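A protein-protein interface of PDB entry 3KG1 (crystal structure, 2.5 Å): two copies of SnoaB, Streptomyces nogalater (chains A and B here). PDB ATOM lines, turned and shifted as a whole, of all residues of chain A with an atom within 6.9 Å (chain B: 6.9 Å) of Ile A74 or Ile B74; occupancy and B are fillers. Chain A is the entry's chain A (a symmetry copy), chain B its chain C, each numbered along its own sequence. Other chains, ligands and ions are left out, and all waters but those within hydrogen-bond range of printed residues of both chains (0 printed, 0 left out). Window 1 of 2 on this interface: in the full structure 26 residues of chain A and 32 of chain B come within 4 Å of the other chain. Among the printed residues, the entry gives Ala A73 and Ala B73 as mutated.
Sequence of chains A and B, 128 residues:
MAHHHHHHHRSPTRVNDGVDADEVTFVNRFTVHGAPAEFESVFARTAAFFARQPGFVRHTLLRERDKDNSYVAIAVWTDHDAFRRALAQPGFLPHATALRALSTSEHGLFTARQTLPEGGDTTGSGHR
Ile A74 touches one residue of chain B. Ile B74 touches just one residue of chain A: Ile A74 (3.7 Å). Printed residues of chain B within 4 Å of Thr A25: Leu B62 (3.95 Å). Of the printed residues of chain A, Arg B58 touches Leu A116. His A59 touches none of the printed residues of chain B.
Among the printed residues, pairs that only touch across the chains: Leu A116 with Arg B58 (3.3 Å), Ile A74 with Ile B74 (3.7 Å), Leu A62 with Thr B25 (3.8 Å), Leu A62 with Val B27 (3.9 Å) and Thr A25 with Leu B62 (3.95 Å).
The backbone NH (N) of His B59 lies within hydrogen-bond range of the backbone carbonyl oxygen (O) of Leu A116, at 2.7 Å.
Thr A25 touches Leu B62, and with the chains exchanged Leu A62 touches Thr B25. Leu A62 touches Val B27, but with the chains exchanged Val A27 does not touch Leu B62 (4.1 Å). Ile B74 touches its own counterpart, Ile A74. Of the 6 pairs that touch across the chains among the printed residues, 3 have their exchanged pair printed and touching as well.
The backbone NH (N) of Leu A62 lies within hydrogen-bond range of the backbone carbonyl oxygen (O) of Val A72 (2.7 Å). The backbone NH (N) of Thr A60 sits at hydrogen-bond distance from the backbone carbonyl oxygen (O) of Ile A74. O of Arg B58 is in hydrogen-bond range of N of Val B76 (2.9 Å). The backbone NH (N) of Leu B62 sits at hydrogen-bond distance from the backbone carbonyl oxygen (O) of Val B72 (2.8 Å). The backbone NH (N) of Thr B60 lies within hydrogen-bond range of the backbone carbonyl oxygen (O) of Ile B74, at 2.9 Å.
Of the 17 printed residues of chain A, 4 touch a printed residue of chain B. Printed residues of chain A that touch a printed residue of chain B: Thr A25, Leu A62, Ile A74 and Leu A116. Hydrophobic or aromatic side chains of chain A within 4 Å of the printed part of chain B: Leu A62 and Ile A74. Of the 17 printed residues of chain B, 6 touch a printed residue of chain A. Among the printed residues, no Asp or Glu carboxylate lies within 4 Å of a Lys or Arg side-chain nitrogen of the other chain.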
ATOM      1  N   THR A  25     -15.513  -4.977  23.687  1.00  0.00           N
ATOM      2  CA  THR A  25     -16.190  -5.925  22.829  1.00  0.00           C
ATOM      3  C   THR A  25     -17.670  -5.672  22.945  1.00  0.00           C
ATOM      4  O   THR A  25     -18.253  -5.809  24.011  1.00  0.00           O
ATOM      5  CB  THR A  25     -15.910  -7.363  23.268  1.00  0.00           C
ATOM      6  OG1 THR A  25     -14.504  -7.600  23.166  1.00  0.00           O
ATOM      7  CG2 THR A  25     -16.686  -8.363  22.400  1.00  0.00           C
ATOM      8  N   PHE A  26     -18.257  -5.284  21.830  1.00  0.00           N
ATOM      9  CA  PHE A  26     -19.694  -5.118  21.711  1.00  0.00           C
ATOM     10  C   PHE A  26     -20.381  -6.459  21.353  1.00  0.00           C
ATOM     11  O   PHE A  26     -20.049  -7.042  20.353  1.00  0.00           O
ATOM     12  CB  PHE A  26     -19.947  -4.079  20.627  1.00  0.00           C
ATOM     13  CG  PHE A  26     -21.341  -3.599  20.577  1.00  0.00           C
ATOM     14  CD1 PHE A  26     -21.889  -2.926  21.651  1.00  0.00           C
ATOM     15  CD2 PHE A  26     -22.116  -3.813  19.457  1.00  0.00           C
ATOM     16  CE1 PHE A  26     -23.203  -2.481  21.605  1.00  0.00           C
ATOM     17  CE2 PHE A  26     -23.429  -3.381  19.418  1.00  0.00           C
ATOM     18  CZ  PHE A  26     -23.972  -2.718  20.489  1.00  0.00           C
ATOM     19  N   VAL A  27     -21.301  -6.941  22.183  1.00  0.00           N
ATOM     20  CA  VAL A  27     -22.059  -8.172  21.884  1.00  0.00           C
ATOM     21  C   VAL A  27     -23.500  -7.794  21.649  1.00  0.00           C
ATOM     22  O   VAL A  27     -24.100  -7.134  22.486  1.00  0.00           O
ATOM     23  CB  VAL A  27     -22.036  -9.245  23.034  1.00  0.00           C
ATOM     24  CG1 VAL A  27     -22.946 -10.426  22.675  1.00  0.00           C
ATOM     25  CG2 VAL A  27     -20.619  -9.762  23.303  1.00  0.00           C
ATOM     26  N   ASN A  28     -24.048  -8.208  20.514  1.00  0.00           N
ATOM     27  CA  ASN A  28     -25.402  -7.846  20.116  1.00  0.00           C
ATOM     28  C   ASN A  28     -26.203  -9.103  19.730  1.00  0.00           C
ATOM     29  O   ASN A  28     -25.902  -9.749  18.743  1.00  0.00           O
ATOM     30  CB  ASN A  28     -25.318  -6.875  18.926  1.00  0.00           C
ATOM     31  CG  ASN A  28     -26.607  -6.089  18.699  1.00  0.00           C
ATOM     32  OD1 ASN A  28     -27.708  -6.531  19.073  1.00  0.00           O
ATOM     33  ND2 ASN A  28     -26.477  -4.917  18.079  1.00  0.00           N
ATOM     34  N   PHE A  43     -26.731  -6.713   7.535  1.00  0.00           N
ATOM     35  CA  PHE A  43     -25.586  -6.859   8.421  1.00  0.00           C
ATOM     36  C   PHE A  43     -24.212  -6.672   7.781  1.00  0.00           C
ATOM     37  O   PHE A  43     -23.355  -6.003   8.340  1.00  0.00           O
ATOM     38  CB  PHE A  43     -25.564  -8.202   9.095  1.00  0.00           C
ATOM     39  CG  PHE A  43     -24.704  -8.203  10.276  1.00  0.00           C
ATOM     40  CD1 PHE A  43     -25.203  -7.775  11.484  1.00  0.00           C
ATOM     41  CD2 PHE A  43     -23.360  -8.534  10.173  1.00  0.00           C
ATOM     42  CE1 PHE A  43     -24.386  -7.724  12.607  1.00  0.00           C
ATOM     43  CE2 PHE A  43     -22.527  -8.499  11.293  1.00  0.00           C
ATOM     44  CZ  PHE A  43     -23.039  -8.094  12.508  1.00  0.00           C
ATOM     45  N   PHE A  56     -11.005  -0.147  14.821  1.00  0.00           N
ATOM     46  CA  PHE A  56     -11.670  -1.408  14.579  1.00  0.00           C
ATOM     47  C   PHE A  56     -10.620  -2.519  14.616  1.00  0.00           C
ATOM     48  O   PHE A  56      -9.501  -2.338  14.100  1.00  0.00           O
ATOM     49  CB  PHE A  56     -12.404  -1.377  13.240  1.00  0.00           C
ATOM     50  CG  PHE A  56     -13.124  -2.648  12.916  1.00  0.00           C
ATOM     51  CD1 PHE A  56     -14.384  -2.912  13.464  1.00  0.00           C
ATOM     52  CD2 PHE A  56     -12.548  -3.591  12.059  1.00  0.00           C
ATOM     53  CE1 PHE A  56     -15.076  -4.110  13.156  1.00  0.00           C
ATOM     54  CE2 PHE A  56     -13.229  -4.791  11.742  1.00  0.00           C
ATOM     55  CZ  PHE A  56     -14.488  -5.045  12.295  1.00  0.00           C
ATOM     56  N   ARG A  58     -11.894  -6.422  14.985  1.00  0.00           N
ATOM     57  CA  ARG A  58     -12.586  -7.527  14.288  1.00  0.00           C
ATOM     58  C   ARG A  58     -14.090  -7.613  14.598  1.00  0.00           C
ATOM     59  O   ARG A  58     -14.616  -6.879  15.429  1.00  0.00           O
ATOM     60  CB  ARG A  58     -11.909  -8.870  14.587  1.00  0.00           C
ATOM     61  CG  ARG A  58     -12.115  -9.335  16.010  1.00  0.00           C
ATOM     62  CD  ARG A  58     -11.421 -10.679  16.357  1.00  0.00           C
ATOM     63  NE  ARG A  58     -10.989 -10.612  17.758  1.00  0.00           N
ATOM     64  CZ  ARG A  58      -9.780 -10.198  18.165  1.00  0.00           C
ATOM     65  NH1 ARG A  58      -8.832  -9.853  17.285  1.00  0.00           N
ATOM     66  NH2 ARG A  58      -9.506 -10.135  19.475  1.00  0.00           N
ATOM     67  N   HIS A  59     -14.773  -8.510  13.891  1.00  0.00           N
ATOM     68  CA  HIS A  59     -16.222  -8.670  13.977  1.00  0.00           C
ATOM     69  C   HIS A  59     -16.598 -10.107  13.620  1.00  0.00           C
ATOM     70  O   HIS A  59     -16.067 -10.666  12.670  1.00  0.00           O
ATOM     71  CB  HIS A  59     -16.950  -7.696  13.031  1.00  0.00           C
ATOM     72  N   THR A  60     -17.512 -10.699  14.376  1.00  0.00           N
ATOM     73  CA  THR A  60     -18.014 -12.044  14.056  1.00  0.00           C
ATOM     74  C   THR A  60     -19.534 -12.045  14.085  1.00  0.00           C
ATOM     75  O   THR A  60     -20.132 -11.438  14.973  1.00  0.00           O
ATOM     76  CB  THR A  60     -17.469 -13.104  15.030  1.00  0.00           C
ATOM     77  OG1 THR A  60     -16.084 -12.842  15.269  1.00  0.00           O
ATOM     78  CG2 THR A  60     -17.606 -14.516  14.436  1.00  0.00           C
ATOM     79  N   LEU A  61     -20.138 -12.688  13.088  1.00  0.00           N
ATOM     80  CA  LEU A  61     -21.566 -12.980  13.105  1.00  0.00           C
ATOM     81  C   LEU A  61     -21.761 -14.468  13.353  1.00  0.00           C
ATOM     82  O   LEU A  61     -21.166 -15.288  12.674  1.00  0.00           O
ATOM     83  CB  LEU A  61     -22.242 -12.611  11.782  1.00  0.00           C
ATOM     84  CG  LEU A  61     -23.780 -12.724  11.778  1.00  0.00           C
ATOM     85  CD1 LEU A  61     -24.383 -11.755  12.782  1.00  0.00           C
ATOM     86  CD2 LEU A  61     -24.365 -12.480  10.400  1.00  0.00           C
ATOM     87  N   LEU A  62     -22.621 -14.793  14.316  1.00  0.00           N
ATOM     88  CA  LEU A  62     -22.906 -16.150  14.733  1.00  0.00           C
ATOM     89  C   LEU A  62     -24.384 -16.467  14.498  1.00  0.00           C
ATOM     90  O   LEU A  62     -25.253 -15.641  14.744  1.00  0.00           O
ATOM     91  CB  LEU A  62     -22.579 -16.286  16.233  1.00  0.00           C
ATOM     92  CG  LEU A  62     -21.123 -16.018  16.684  1.00  0.00           C
ATOM     93  CD1 LEU A  62     -20.973 -16.123  18.198  1.00  0.00           C
ATOM     94  CD2 LEU A  62     -20.145 -16.963  16.005  1.00  0.00           C
ATOM     95  N   VAL A  72     -25.992 -13.642  16.909  1.00  0.00           N
ATOM     96  CA  VAL A  72     -25.165 -12.902  17.842  1.00  0.00           C
ATOM     97  C   VAL A  72     -24.030 -12.301  17.024  1.00  0.00           C
ATOM     98  O   VAL A  72     -23.392 -13.011  16.250  1.00  0.00           O
ATOM     99  CB  VAL A  72     -24.593 -13.800  18.993  1.00  0.00           C
ATOM    100  CG1 VAL A  72     -23.616 -13.004  19.874  1.00  0.00           C
ATOM    101  CG2 VAL A  72     -25.701 -14.368  19.842  1.00  0.00           C
ATOM    102  N   ALA A  73     -23.815 -10.994  17.176  1.00  0.00           N
ATOM    103  CA  ALA A  73     -22.654 -10.315  16.609  1.00  0.00           C
ATOM    104  C   ALA A  73     -21.702  -9.939  17.714  1.00  0.00           C
ATOM    105  O   ALA A  73     -22.107  -9.724  18.852  1.00  0.00           O
ATOM    106  CB  ALA A  73     -23.051  -9.086  15.844  1.00  0.00           C
ATOM    107  N   ILE A  74     -20.427  -9.818  17.369  1.00  0.00           N
ATOM    108  CA  ILE A  74     -19.383  -9.535  18.352  1.00  0.00           C
ATOM    109  C   ILE A  74     -18.406  -8.595  17.651  1.00  0.00           C
ATOM    110  O   ILE A  74     -17.857  -8.932  16.594  1.00  0.00           O
ATOM    111  CB  ILE A  74     -18.692 -10.859  18.830  1.00  0.00           C
ATOM    112  CG1 ILE A  74     -19.748 -11.889  19.298  1.00  0.00           C
ATOM    113  CG2 ILE A  74     -17.701 -10.591  19.950  1.00  0.00           C
ATOM    114  CD1 ILE A  74     -19.146 -13.165  19.830  1.00  0.00           C
ATOM    115  N   ALA A  75     -18.235  -7.398  18.192  1.00  0.00           N
ATOM    116  CA  ALA A  75     -17.359  -6.422  17.574  1.00  0.00           C
ATOM    117  C   ALA A  75     -16.290  -5.974  18.587  1.00  0.00           C
ATOM    118  O   ALA A  75     -16.606  -5.500  19.689  1.00  0.00           O
ATOM    119  CB  ALA A  75     -18.169  -5.213  17.050  1.00  0.00           C
ATOM    120  N   VAL A  76     -15.027  -6.161  18.218  1.00  0.00           N
ATOM    121  CA  VAL A  76     -13.952  -5.712  19.062  1.00  0.00           C
ATOM    122  C   VAL A  76     -13.412  -4.358  18.583  1.00  0.00           C
ATOM    123  O   VAL A  76     -13.152  -4.176  17.390  1.00  0.00           O
ATOM    124  CB  VAL A  76     -12.814  -6.671  19.066  1.00  0.00           C
ATOM    125  CG1 VAL A  76     -11.719  -6.125  19.990  1.00  0.00           C
ATOM    126  CG2 VAL A  76     -13.288  -8.048  19.504  1.00  0.00           C
ATOM    127  N   LEU A 116      -7.716 -17.348  25.882  1.00  0.00           N
ATOM    128  CA  LEU A 116      -6.820 -18.469  25.582  1.00  0.00           C
ATOM    129  C   LEU A 116      -7.115 -18.983  24.165  1.00  0.00           C
ATOM    130  O   LEU A 116      -8.287 -19.155  23.821  1.00  0.00           O
ATOM    131  CB  LEU A 116      -7.008 -19.625  26.576  1.00  0.00           C
ATOM    132  CG  LEU A 116      -6.217 -19.733  27.881  1.00  0.00           C
ATOM    133  CD1 LEU A 116      -6.654 -20.996  28.601  1.00  0.00           C
ATOM    134  CD2 LEU A 116      -4.749 -19.799  27.621  1.00  0.00           C
ATOM    135  N   THR B  25     -19.301 -22.383  17.854  1.00  0.00           N
ATOM    136  CA  THR B  25     -19.000 -21.367  18.862  1.00  0.00           C
ATOM    137  C   THR B  25     -20.062 -21.441  19.938  1.00  0.00           C
ATOM    138  O   THR B  25     -21.192 -21.070  19.709  1.00  0.00           O
ATOM    139  CB  THR B  25     -18.946 -19.965  18.260  1.00  0.00           C
ATOM    140  OG1 THR B  25     -17.945 -19.942  17.234  1.00  0.00           O
ATOM    141  CG2 THR B  25     -18.635 -18.910  19.338  1.00  0.00           C
ATOM    142  N   PHE B  26     -19.686 -21.957  21.100  1.00  0.00           N
ATOM    143  CA  PHE B  26     -20.573 -22.075  22.239  1.00  0.00           C
ATOM    144  C   PHE B  26     -20.611 -20.763  22.963  1.00  0.00           C
ATOM    145  O   PHE B  26     -19.549 -20.208  23.286  1.00  0.00           O
ATOM    146  CB  PHE B  26     -20.024 -23.150  23.154  1.00  0.00           C
ATOM    147  CG  PHE B  26     -20.842 -23.409  24.374  1.00  0.00           C
ATOM    148  CD1 PHE B  26     -22.155 -23.830  24.272  1.00  0.00           C
ATOM    149  CD2 PHE B  26     -20.267 -23.309  25.633  1.00  0.00           C
ATOM    150  CE1 PHE B  26     -22.904 -24.122  25.420  1.00  0.00           C
ATOM    151  CE2 PHE B  26     -20.999 -23.582  26.766  1.00  0.00           C
ATOM    152  CZ  PHE B  26     -22.327 -24.009  26.660  1.00  0.00           C
ATOM    153  N   VAL B  27     -21.810 -20.234  23.186  1.00  0.00           N
ATOM    154  CA  VAL B  27     -21.975 -18.947  23.878  1.00  0.00           C
ATOM    155  C   VAL B  27     -22.843 -19.192  25.108  1.00  0.00           C
ATOM    156  O   VAL B  27     -23.960 -19.733  25.008  1.00  0.00           O
ATOM    157  CB  VAL B  27     -22.614 -17.863  22.976  1.00  0.00           C
ATOM    158  CG1 VAL B  27     -22.753 -16.560  23.737  1.00  0.00           C
ATOM    159  CG2 VAL B  27     -21.791 -17.650  21.719  1.00  0.00           C
ATOM    160  N   ASN B  28     -22.315 -18.799  26.257  1.00  0.00           N
ATOM    161  CA  ASN B  28     -22.899 -19.087  27.549  1.00  0.00           C
ATOM    162  C   ASN B  28     -22.971 -17.813  28.414  1.00  0.00           C
ATOM    163  O   ASN B  28     -21.932 -17.199  28.712  1.00  0.00           O
ATOM    164  CB  ASN B  28     -22.008 -20.116  28.210  1.00  0.00           C
ATOM    165  CG  ASN B  28     -22.679 -20.848  29.320  1.00  0.00           C
ATOM    166  OD1 ASN B  28     -23.782 -20.497  29.747  1.00  0.00           O
ATOM    167  ND2 ASN B  28     -22.013 -21.873  29.812  1.00  0.00           N
ATOM    168  N   PHE B  43     -13.287 -20.271  36.496  1.00  0.00           N
ATOM    169  CA  PHE B  43     -13.278 -20.238  35.033  1.00  0.00           C
ATOM    170  C   PHE B  43     -11.894 -20.429  34.388  1.00  0.00           C
ATOM    171  O   PHE B  43     -11.787 -21.122  33.375  1.00  0.00           O
ATOM    172  CB  PHE B  43     -13.982 -19.007  34.445  1.00  0.00           C
ATOM    173  CG  PHE B  43     -14.993 -19.380  33.382  1.00  0.00           C
ATOM    174  CD1 PHE B  43     -16.343 -19.172  33.578  1.00  0.00           C
ATOM    175  CD2 PHE B  43     -14.598 -20.046  32.241  1.00  0.00           C
ATOM    176  CE1 PHE B  43     -17.260 -19.571  32.629  1.00  0.00           C
ATOM    177  CE2 PHE B  43     -15.536 -20.453  31.288  1.00  0.00           C
ATOM    178  CZ  PHE B  43     -16.856 -20.208  31.488  1.00  0.00           C
ATOM    179  N   PHE B  56     -10.034 -27.985  20.515  1.00  0.00           N
ATOM    180  CA  PHE B  56     -10.186 -26.685  21.170  1.00  0.00           C
ATOM    181  C   PHE B  56      -9.556 -25.637  20.284  1.00  0.00           C
ATOM    182  O   PHE B  56      -8.392 -25.750  19.948  1.00  0.00           O
ATOM    183  CB  PHE B  56      -9.494 -26.676  22.538  1.00  0.00           C
ATOM    184  CG  PHE B  56      -9.627 -25.374  23.273  1.00  0.00           C
ATOM    185  CD1 PHE B  56     -10.833 -24.988  23.817  1.00  0.00           C
ATOM    186  CD2 PHE B  56      -8.539 -24.515  23.398  1.00  0.00           C
ATOM    187  CE1 PHE B  56     -10.956 -23.759  24.468  1.00  0.00           C
ATOM    188  CE2 PHE B  56      -8.658 -23.310  24.074  1.00  0.00           C
ATOM    189  CZ  PHE B  56      -9.870 -22.937  24.593  1.00  0.00           C
ATOM    190  N   ARG B  58     -10.411 -21.710  20.656  1.00  0.00           N
ATOM    191  CA  ARG B  58     -10.144 -20.559  21.527  1.00  0.00           C
ATOM    192  C   ARG B  58     -11.211 -20.345  22.569  1.00  0.00           C
ATOM    193  O   ARG B  58     -12.266 -20.961  22.520  1.00  0.00           O
ATOM    194  CB  ARG B  58      -9.881 -19.281  20.716  1.00  0.00           C
ATOM    195  CG  ARG B  58     -11.074 -18.610  20.085  1.00  0.00           C
ATOM    196  CD  ARG B  58     -10.651 -17.390  19.217  1.00  0.00           C
ATOM    197  NE  ARG B  58     -11.545 -17.264  18.062  1.00  0.00           N
ATOM    198  CZ  ARG B  58     -11.336 -17.805  16.861  1.00  0.00           C
ATOM    199  NH1 ARG B  58     -10.233 -18.515  16.589  1.00  0.00           N
ATOM    200  NH2 ARG B  58     -12.239 -17.635  15.910  1.00  0.00           N
ATOM    201  N   HIS B  59     -10.910 -19.502  23.547  1.00  0.00           N
ATOM    202  CA  HIS B  59     -11.854 -19.207  24.625  1.00  0.00           C
ATOM    203  C   HIS B  59     -11.685 -17.779  25.132  1.00  0.00           C
ATOM    204  O   HIS B  59     -10.565 -17.326  25.364  1.00  0.00           O
ATOM    205  CB  HIS B  59     -11.656 -20.178  25.789  1.00  0.00           C
ATOM    206  CG  HIS B  59     -11.783 -19.537  27.132  1.00  0.00           C
ATOM    207  ND1 HIS B  59     -12.998 -19.382  27.774  1.00  0.00           N
ATOM    208  CD2 HIS B  59     -10.849 -18.981  27.943  1.00  0.00           C
ATOM    209  CE1 HIS B  59     -12.801 -18.752  28.923  1.00  0.00           C
ATOM    210  NE2 HIS B  59     -11.508 -18.490  29.047  1.00  0.00           N
ATOM    211  N   THR B  60     -12.803 -17.080  25.310  1.00  0.00           N
ATOM    212  CA  THR B  60     -12.784 -15.757  25.939  1.00  0.00           C
ATOM    213  C   THR B  60     -13.831 -15.726  27.037  1.00  0.00           C
ATOM    214  O   THR B  60     -14.914 -16.292  26.875  1.00  0.00           O
ATOM    215  CB  THR B  60     -13.093 -14.636  24.945  1.00  0.00           C
ATOM    216  OG1 THR B  60     -12.278 -14.803  23.792  1.00  0.00           O
ATOM    217  CG2 THR B  60     -12.798 -13.296  25.563  1.00  0.00           C
ATOM    218  N   LEU B  61     -13.478 -15.103  28.159  1.00  0.00           N
ATOM    219  CA  LEU B  61     -14.449 -14.742  29.176  1.00  0.00           C
ATOM    220  C   LEU B  61     -14.592 -13.205  29.204  1.00  0.00           C
ATOM    221  O   LEU B  61     -13.623 -12.461  29.454  1.00  0.00           O
ATOM    222  CB  LEU B  61     -14.058 -15.293  30.544  1.00  0.00           C
ATOM    223  CG  LEU B  61     -15.046 -15.010  31.685  1.00  0.00           C
ATOM    224  CD1 LEU B  61     -16.337 -15.790  31.506  1.00  0.00           C
ATOM    225  CD2 LEU B  61     -14.397 -15.340  33.021  1.00  0.00           C
ATOM    226  N   LEU B  62     -15.810 -12.753  28.918  1.00  0.00           N
ATOM    227  CA  LEU B  62     -16.150 -11.344  28.882  1.00  0.00           C
ATOM    228  C   LEU B  62     -16.973 -10.965  30.111  1.00  0.00           C
ATOM    229  O   LEU B  62     -17.666 -11.795  30.686  1.00  0.00           O
ATOM    230  CB  LEU B  62     -16.898 -11.019  27.596  1.00  0.00           C
ATOM    231  CG  LEU B  62     -16.195 -11.282  26.241  1.00  0.00           C
ATOM    232  CD1 LEU B  62     -17.243 -11.182  25.112  1.00  0.00           C
ATOM    233  CD2 LEU B  62     -15.012 -10.336  25.988  1.00  0.00           C
ATOM    234  N   VAL B  72     -20.072 -13.287  29.784  1.00  0.00           N
ATOM    235  CA  VAL B  72     -20.355 -14.125  28.628  1.00  0.00           C
ATOM    236  C   VAL B  72     -19.088 -14.907  28.312  1.00  0.00           C
ATOM    237  O   VAL B  72     -18.007 -14.346  28.270  1.00  0.00           O
ATOM    238  CB  VAL B  72     -20.869 -13.312  27.440  1.00  0.00           C
ATOM    239  CG1 VAL B  72     -21.253 -14.203  26.307  1.00  0.00           C
ATOM    240  CG2 VAL B  72     -22.061 -12.500  27.863  1.00  0.00           C
ATOM    241  N   ALA B  73     -19.230 -16.222  28.163  1.00  0.00           N
ATOM    242  CA  ALA B  73     -18.107 -17.081  27.814  1.00  0.00           C
ATOM    243  C   ALA B  73     -18.362 -17.611  26.427  1.00  0.00           C
ATOM    244  O   ALA B  73     -19.439 -18.119  26.128  1.00  0.00           O
ATOM    245  CB  ALA B  73     -17.920 -18.209  28.803  1.00  0.00           C
ATOM    246  N   ILE B  74     -17.335 -17.468  25.602  1.00  0.00           N
ATOM    247  CA  ILE B  74     -17.344 -17.801  24.195  1.00  0.00           C
ATOM    248  C   ILE B  74     -16.256 -18.842  23.984  1.00  0.00           C
ATOM    249  O   ILE B  74     -15.108 -18.566  24.258  1.00  0.00           O
ATOM    250  CB  ILE B  74     -17.071 -16.553  23.356  1.00  0.00           C
ATOM    251  CG1 ILE B  74     -18.148 -15.503  23.642  1.00  0.00           C
ATOM    252  CG2 ILE B  74     -17.061 -16.900  21.900  1.00  0.00           C
ATOM    253  CD1 ILE B  74     -17.821 -14.115  23.116  1.00  0.00           C
ATOM    254  N   ALA B  75     -16.630 -20.053  23.563  1.00  0.00           N
ATOM    255  CA  ALA B  75     -15.665 -21.163  23.365  1.00  0.00           C
ATOM    256  C   ALA B  75     -15.799 -21.676  21.933  1.00  0.00           C
ATOM    257  O   ALA B  75     -16.900 -21.919  21.475  1.00  0.00           O
ATOM    258  CB  ALA B  75     -15.892 -22.276  24.357  1.00  0.00           C
ATOM    259  N   VAL B  76     -14.685 -21.790  21.216  1.00  0.00           N
ATOM    260  CA  VAL B  76     -14.730 -22.245  19.838  1.00  0.00           C
ATOM    261  C   VAL B  76     -14.145 -23.640  19.757  1.00  0.00           C
ATOM    262  O   VAL B  76     -13.146 -23.922  20.368  1.00  0.00           O
ATOM    263  CB  VAL B  76     -14.082 -21.249  18.848  1.00  0.00           C
ATOM    264  CG1 VAL B  76     -14.276 -21.709  17.377  1.00  0.00           C
ATOM    265  CG2 VAL B  76     -14.681 -19.850  19.054  1.00  0.00           C
ATOM    266  N   TRP B  77     -14.832 -24.509  19.014  1.00  0.00           N
ATOM    267  CA  TRP B  77     -14.449 -25.893  18.846  1.00  0.00           C
ATOM    268  C   TRP B  77     -14.496 -26.225  17.371  1.00  0.00           C
ATOM    269  O   TRP B  77     -15.326 -25.685  16.652  1.00  0.00           O
ATOM    270  CB  TRP B  77     -15.397 -26.796  19.652  1.00  0.00           C
ATOM    271  CG  TRP B  77     -15.312 -26.515  21.105  1.00  0.00           C
ATOM    272  CD1 TRP B  77     -16.000 -25.568  21.795  1.00  0.00           C
ATOM    273  CD2 TRP B  77     -14.467 -27.170  22.054  1.00  0.00           C
ATOM    274  NE1 TRP B  77     -15.658 -25.599  23.119  1.00  0.00           N
ATOM    275  CE2 TRP B  77     -14.706 -26.567  23.308  1.00  0.00           C
ATOM    276  CE3 TRP B  77     -13.537 -28.225  21.973  1.00  0.00           C
ATOM    277  CZ2 TRP B  77     -14.047 -26.971  24.472  1.00  0.00           C
ATOM    278  CZ3 TRP B  77     -12.887 -28.631  23.136  1.00  0.00           C
ATOM    279  CH2 TRP B  77     -13.146 -27.996  24.371  1.00  0.00           C
